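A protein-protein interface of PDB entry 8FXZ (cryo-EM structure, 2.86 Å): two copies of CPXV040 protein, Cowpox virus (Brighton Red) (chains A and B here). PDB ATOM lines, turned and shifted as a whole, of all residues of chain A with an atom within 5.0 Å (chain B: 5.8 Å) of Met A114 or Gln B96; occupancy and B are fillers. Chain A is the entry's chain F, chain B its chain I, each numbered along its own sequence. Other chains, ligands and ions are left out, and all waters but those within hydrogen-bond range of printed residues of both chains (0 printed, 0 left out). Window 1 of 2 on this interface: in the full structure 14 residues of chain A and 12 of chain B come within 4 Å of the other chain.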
ATOM      1  N   TYR A  32      19.027 -30.633   9.008  1.00  0.00           N
ATOM      2  CA  TYR A  32      17.656 -31.052   8.783  1.00  0.00           C
ATOM      3  C   TYR A  32      17.422 -31.231   7.291  1.00  0.00           C
ATOM      4  O   TYR A  32      18.246 -30.846   6.458  1.00  0.00           O
ATOM      5  CB  TYR A  32      16.670 -30.052   9.385  1.00  0.00           C
ATOM      6  CG  TYR A  32      16.586 -28.722   8.692  1.00  0.00           C
ATOM      7  CD1 TYR A  32      17.441 -27.689   9.019  1.00  0.00           C
ATOM      8  CD2 TYR A  32      15.620 -28.486   7.737  1.00  0.00           C
ATOM      9  CE1 TYR A  32      17.349 -26.477   8.395  1.00  0.00           C
ATOM     10  CE2 TYR A  32      15.527 -27.282   7.112  1.00  0.00           C
ATOM     11  CZ  TYR A  32      16.387 -26.280   7.449  1.00  0.00           C
ATOM     12  OH  TYR A  32      16.291 -25.068   6.819  1.00  0.00           O
ATOM     13  N   CYS A 111      17.997 -19.573  11.601  1.00  0.00           N
ATOM     14  CA  CYS A 111      17.112 -20.694  11.325  1.00  0.00           C
ATOM     15  C   CYS A 111      15.674 -20.325  11.654  1.00  0.00           C
ATOM     16  O   CYS A 111      15.399 -19.736  12.700  1.00  0.00           O
ATOM     17  CB  CYS A 111      17.512 -21.913  12.137  1.00  0.00           C
ATOM     18  SG  CYS A 111      19.220 -22.390  12.025  1.00  0.00           S
ATOM     19  N   MET A 112      14.755 -20.706  10.770  1.00  0.00           N
ATOM     20  CA  MET A 112      13.360 -20.324  10.896  1.00  0.00           C
ATOM     21  C   MET A 112      12.400 -21.494  11.044  1.00  0.00           C
ATOM     22  O   MET A 112      11.259 -21.272  11.461  1.00  0.00           O
ATOM     23  CB  MET A 112      12.923 -19.493   9.682  1.00  0.00           C
ATOM     24  CG  MET A 112      13.800 -18.295   9.375  1.00  0.00           C
ATOM     25  SD  MET A 112      13.659 -16.942  10.548  1.00  0.00           S
ATOM     26  CE  MET A 112      11.983 -16.395  10.244  1.00  0.00           C
ATOM     27  N   GLU A 113      12.809 -22.712  10.726  1.00  0.00           N
ATOM     28  CA  GLU A 113      11.887 -23.843  10.748  1.00  0.00           C
ATOM     29  C   GLU A 113      12.368 -25.009  11.596  1.00  0.00           C
ATOM     30  O   GLU A 113      11.544 -25.668  12.232  1.00  0.00           O
ATOM     31  CB  GLU A 113      11.628 -24.323   9.323  1.00  0.00           C
ATOM     32  CG  GLU A 113      10.747 -23.394   8.524  1.00  0.00           C
ATOM     33  CD  GLU A 113      10.445 -23.923   7.142  1.00  0.00           C
ATOM     34  OE1 GLU A 113      11.196 -24.794   6.660  1.00  0.00           O
ATOM     35  OE2 GLU A 113       9.456 -23.469   6.536  1.00  0.00           O
ATOM     36  N   MET A 114      13.666 -25.287  11.621  1.00  0.00           N
ATOM     37  CA  MET A 114      14.207 -26.344  12.459  1.00  0.00           C
ATOM     38  C   MET A 114      15.413 -25.834  13.227  1.00  0.00           C
ATOM     39  O   MET A 114      16.171 -24.993  12.742  1.00  0.00           O
ATOM     40  CB  MET A 114      14.601 -27.566  11.640  1.00  0.00           C
ATOM     41  CG  MET A 114      13.442 -28.226  10.934  1.00  0.00           C
ATOM     42  SD  MET A 114      12.382 -29.176  12.030  1.00  0.00           S
ATOM     43  CE  MET A 114      13.388 -30.624  12.287  1.00  0.00           C
ATOM     44  N   ASN A 115      15.563 -26.348  14.441  1.00  0.00           N
ATOM     45  CA  ASN A 115      16.728 -26.092  15.280  1.00  0.00           C
ATOM     46  C   ASN A 115      16.968 -24.597  15.485  1.00  0.00           C
ATOM     47  O   ASN A 115      18.088 -24.103  15.383  1.00  0.00           O
ATOM     48  CB  ASN A 115      17.954 -26.783  14.698  1.00  0.00           C
ATOM     49  CG  ASN A 115      17.882 -28.283  14.835  1.00  0.00           C
ATOM     50  OD1 ASN A 115      18.424 -28.855  15.777  1.00  0.00           O
ATOM     51  ND2 ASN A 115      17.203 -28.930  13.902  1.00  0.00           N
ATOM     52  N   CYS A 116      15.903 -23.883  15.812  1.00  0.00           N
ATOM     53  CA  CYS A 116      15.990 -22.466  16.112  1.00  0.00           C
ATOM     54  C   CYS A 116      16.607 -22.243  17.487  1.00  0.00           C
ATOM     55  O   CYS A 116      16.610 -23.127  18.345  1.00  0.00           O
ATOM     56  CB  CYS A 116      14.610 -21.831  16.049  1.00  0.00           C
ATOM     57  SG  CYS A 116      13.675 -22.290  14.587  1.00  0.00           S
ATOM     58  N   CYS A 143      21.427 -25.291  13.335  1.00  0.00           N
ATOM     59  CA  CYS A 143      21.049 -25.977  12.112  1.00  0.00           C
ATOM     60  C   CYS A 143      22.149 -26.005  11.073  1.00  0.00           C
ATOM     61  O   CYS A 143      22.065 -26.798  10.132  1.00  0.00           O
ATOM     62  CB  CYS A 143      19.821 -25.301  11.507  1.00  0.00           C
ATOM     63  SG  CYS A 143      19.087 -24.273  12.747  1.00  0.00           S
ATOM     64  N   CYS B  11      10.519 -22.695  17.322  1.00  0.00           N
ATOM     65  CA  CYS B  11      10.541 -22.022  16.039  1.00  0.00           C
ATOM     66  C   CYS B  11       9.373 -21.042  15.947  1.00  0.00           C
ATOM     67  O   CYS B  11       8.352 -21.218  16.612  1.00  0.00           O
ATOM     68  CB  CYS B  11      10.461 -23.032  14.904  1.00  0.00           C
ATOM     69  SG  CYS B  11       8.993 -24.075  14.955  1.00  0.00           S
ATOM     70  N   TYR B  19       7.463 -29.356   8.634  1.00  0.00           N
ATOM     71  CA  TYR B  19       8.108 -30.388   9.430  1.00  0.00           C
ATOM     72  C   TYR B  19       7.193 -30.748  10.594  1.00  0.00           C
ATOM     73  O   TYR B  19       6.849 -29.885  11.405  1.00  0.00           O
ATOM     74  CB  TYR B  19       9.476 -29.912   9.913  1.00  0.00           C
ATOM     75  CG  TYR B  19      10.404 -29.550   8.778  1.00  0.00           C
ATOM     76  CD1 TYR B  19      10.275 -28.351   8.111  1.00  0.00           C
ATOM     77  CD2 TYR B  19      11.400 -30.416   8.365  1.00  0.00           C
ATOM     78  CE1 TYR B  19      11.108 -28.023   7.076  1.00  0.00           C
ATOM     79  CE2 TYR B  19      12.237 -30.094   7.330  1.00  0.00           C
ATOM     80  CZ  TYR B  19      12.088 -28.898   6.687  1.00  0.00           C
ATOM     81  OH  TYR B  19      12.917 -28.561   5.649  1.00  0.00           O
ATOM     82  N   TYR B  21       5.773 -33.753  13.660  1.00  0.00           N
ATOM     83  CA  TYR B  21       6.229 -34.733  14.632  1.00  0.00           C
ATOM     84  C   TYR B  21       5.034 -35.466  15.210  1.00  0.00           C
ATOM     85  O   TYR B  21       4.099 -34.833  15.705  1.00  0.00           O
ATOM     86  CB  TYR B  21       7.018 -34.056  15.748  1.00  0.00           C
ATOM     87  CG  TYR B  21       7.496 -34.978  16.826  1.00  0.00           C
ATOM     88  CD1 TYR B  21       8.450 -35.939  16.570  1.00  0.00           C
ATOM     89  CD2 TYR B  21       7.021 -34.860  18.116  1.00  0.00           C
ATOM     90  CE1 TYR B  21       8.892 -36.773  17.558  1.00  0.00           C
ATOM     91  CE2 TYR B  21       7.459 -35.689  19.110  1.00  0.00           C
ATOM     92  CZ  TYR B  21       8.395 -36.640  18.828  1.00  0.00           C
ATOM     93  OH  TYR B  21       8.837 -37.470  19.823  1.00  0.00           O
ATOM     94  N   ASP B  72       7.862 -27.050  24.931  1.00  0.00           N
ATOM     95  CA  ASP B  72       8.416 -26.295  23.818  1.00  0.00           C
ATOM     96  C   ASP B  72       7.859 -26.747  22.478  1.00  0.00           C
ATOM     97  O   ASP B  72       8.356 -26.313  21.436  1.00  0.00           O
ATOM     98  CB  ASP B  72       9.937 -26.401  23.816  1.00  0.00           C
ATOM     99  CG  ASP B  72      10.572 -25.697  24.997  1.00  0.00           C
ATOM    100  OD1 ASP B  72      10.053 -24.640  25.410  1.00  0.00           O
ATOM    101  OD2 ASP B  72      11.589 -26.198  25.518  1.00  0.00           O
ATOM    102  N   GLN B  73       6.854 -27.615  22.481  1.00  0.00           N
ATOM    103  CA  GLN B  73       6.193 -28.043  21.263  1.00  0.00           C
ATOM    104  C   GLN B  73       5.087 -27.066  20.890  1.00  0.00           C
ATOM    105  O   GLN B  73       4.858 -26.053  21.549  1.00  0.00           O
ATOM    106  CB  GLN B  73       5.608 -29.441  21.425  1.00  0.00           C
ATOM    107  CG  GLN B  73       6.616 -30.524  21.669  1.00  0.00           C
ATOM    108  CD  GLN B  73       5.974 -31.884  21.714  1.00  0.00           C
ATOM    109  OE1 GLN B  73       4.770 -32.021  21.517  1.00  0.00           O
ATOM    110  NE2 GLN B  73       6.773 -32.905  21.972  1.00  0.00           N
ATOM    111  N   THR B  94       2.745 -32.304  16.141  1.00  0.00           N
ATOM    112  CA  THR B  94       3.283 -31.083  16.711  1.00  0.00           C
ATOM    113  C   THR B  94       4.559 -30.700  15.968  1.00  0.00           C
ATOM    114  O   THR B  94       4.902 -31.291  14.939  1.00  0.00           O
ATOM    115  CB  THR B  94       3.543 -31.270  18.206  1.00  0.00           C
ATOM    116  OG1 THR B  94       4.460 -32.351  18.397  1.00  0.00           O
ATOM    117  CG2 THR B  94       2.258 -31.567  18.944  1.00  0.00           C
ATOM    118  N   THR B  95       5.260 -29.693  16.478  1.00  0.00           N
ATOM    119  CA  THR B  95       6.597 -29.380  15.998  1.00  0.00           C
ATOM    120  C   THR B  95       7.578 -30.352  16.644  1.00  0.00           C
ATOM    121  O   THR B  95       7.186 -31.333  17.281  1.00  0.00           O
ATOM    122  CB  THR B  95       6.952 -27.923  16.280  1.00  0.00           C
ATOM    123  OG1 THR B  95       7.163 -27.734  17.682  1.00  0.00           O
ATOM    124  CG2 THR B  95       5.850 -27.007  15.806  1.00  0.00           C
ATOM    125  N   GLN B  96       8.869 -30.097  16.485  1.00  0.00           N
ATOM    126  CA  GLN B  96       9.880 -31.021  16.969  1.00  0.00           C
ATOM    127  C   GLN B  96       9.973 -30.991  18.487  1.00  0.00           C
ATOM    128  O   GLN B  96       9.565 -30.038  19.148  1.00  0.00           O
ATOM    129  CB  GLN B  96      11.238 -30.682  16.369  1.00  0.00           C
ATOM    130  CG  GLN B  96      11.756 -29.331  16.801  1.00  0.00           C
ATOM    131  CD  GLN B  96      13.017 -28.937  16.088  1.00  0.00           C
ATOM    132  OE1 GLN B  96      13.187 -27.781  15.708  1.00  0.00           O
ATOM    133  NE2 GLN B  96      13.920 -29.889  15.909  1.00  0.00           N
ATOM    134  N   ARG B  97      10.528 -32.063  19.032  1.00  0.00           N
ATOM    135  CA  ARG B  97      10.731 -32.200  20.463  1.00  0.00           C
ATOM    136  C   ARG B  97      12.138 -31.741  20.820  1.00  0.00           C
ATOM    137  O   ARG B  97      13.120 -32.237  20.256  1.00  0.00           O
ATOM    138  CB  ARG B  97      10.521 -33.653  20.878  1.00  0.00           C
ATOM    139  CG  ARG B  97      10.432 -33.863  22.361  1.00  0.00           C
ATOM    140  CD  ARG B  97       9.869 -35.225  22.673  1.00  0.00           C
ATOM    141  NE  ARG B  97       9.840 -35.474  24.107  1.00  0.00           N
ATOM    142  CZ  ARG B  97       8.952 -34.951  24.938  1.00  0.00           C
ATOM    143  NH1 ARG B  97       7.994 -34.147  24.510  1.00  0.00           N
ATOM    144  NH2 ARG B  97       9.033 -35.233  26.233  1.00  0.00           N
ATOM    145  N   LEU B  98      12.237 -30.801  21.756  1.00  0.00           N
ATOM    146  CA  LEU B  98      13.510 -30.190  22.111  1.00  0.00           C
ATOM    147  C   LEU B  98      14.109 -30.752  23.391  1.00  0.00           C
ATOM    148  O   LEU B  98      15.334 -30.830  23.508  1.00  0.00           O
ATOM    149  CB  LEU B  98      13.341 -28.677  22.260  1.00  0.00           C
ATOM    150  CG  LEU B  98      12.820 -27.929  21.039  1.00  0.00           C
ATOM    151  CD1 LEU B  98      12.730 -26.458  21.349  1.00  0.00           C
ATOM    152  CD2 LEU B  98      13.706 -28.167  19.841  1.00  0.00           C
ATOM    153  N   TYR B 169       8.240 -36.932  11.225  1.00  0.00           N
ATOM    154  CA  TYR B 169       9.192 -37.596  12.098  1.00  0.00           C
ATOM    155  C   TYR B 169       8.458 -38.245  13.264  1.00  0.00           C
ATOM    156  O   TYR B 169       7.345 -37.852  13.626  1.00  0.00           O
ATOM    157  CB  TYR B 169      10.242 -36.617  12.621  1.00  0.00           C
ATOM    158  CG  TYR B 169      10.923 -35.824  11.537  1.00  0.00           C
ATOM    159  CD1 TYR B 169      11.919 -36.387  10.758  1.00  0.00           C
ATOM    160  CD2 TYR B 169      10.569 -34.508  11.291  1.00  0.00           C
ATOM    161  CE1 TYR B 169      12.537 -35.668   9.767  1.00  0.00           C
ATOM    162  CE2 TYR B 169      11.182 -33.781  10.302  1.00  0.00           C
ATOM    163  CZ  TYR B 169      12.166 -34.364   9.545  1.00  0.00           C
ATOM    164  OH  TYR B 169      12.783 -33.637   8.558  1.00  0.00           O
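N of Asn A115 is in hydrogen-bond range of OE1 of Gln B96.
The side-chain sulfur of Cys A116 lies within hydrogen-bond range of the backbone carbonyl oxygen of Cys A111 (3.6 Å).
The side-chain sulfur of Cys A143 is disulfide-bonded to the side-chain sulfur of Cys A111, at 2.0 Å.
Among the printed residues, merely in contact across the chains: Tyr A32 with Tyr B19 (3.3 Å), Met A112 with Cys B11 (3.9 Å), Glu A113 with Cys B11 (3.9 Å), Glu A113 with Tyr B19 (3.3 Å), Met A114 with Tyr B19 (3.7 Å), Met A114 with Gln B96 (3.7 Å) and Cys A116 with Cys B11 (3.3 Å).
Met A114 touches two residues of chain B.
Of chain A, only Met A114 (3.7 Å) and Asn A115 (3.1 Å) come within 4 Å of Gln B96.
Of the printed residues of chain A, Tyr B19 touches Tyr A32 (3.3 Å), Glu A113 (3.3 Å) and Met A114 (3.7 Å).
Of the printed residues of chain B, Met A112 touches Cys B11.
Printed residues of chain B within 4 Å of Cys A116: Cys B11 (3.3 Å).
Of the printed residues of chain B, Asn A115 touches Gln B96.
Leu B98 touches none of the printed residues of chain A.
Tyr B21 touches none of the printed residues of chain A.
The nearest residue of chain B that does not touch Met A114 is Tyr B169 (4.3 Å).
The nearest residue of chain A that does not touch Gln B96 is Glu A113 (4.4 Å).
The nearest printed residue of chain B that does not touch Met A112 is Tyr B19 (7.7 Å).
Hydrophobic or aromatic side chains of chain B within 4 Å of the printed part of chain A: Tyr B19.
Along chain B the printed residues that touch a printed residue of chain A span positions 11 to 96.
Of the 8 printed residues of chain A, 6 touch a printed residue of chain B.
Hydrophobic or aromatic side chains of chain A within 4 Å of the printed part of chain B: Tyr A32 and Met A114.
Among the printed residues, 8 pairs touch across the chains.
Among the printed residues, no Asp or Glu carboxylate lies within 4 Å of a Lys or Arg side-chain nitrogen of the other chain.
No position is printed for both chains.
Of the 8 pairs that touch across the chains among the printed residues, none has its exchanged pair printed and touching as well.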
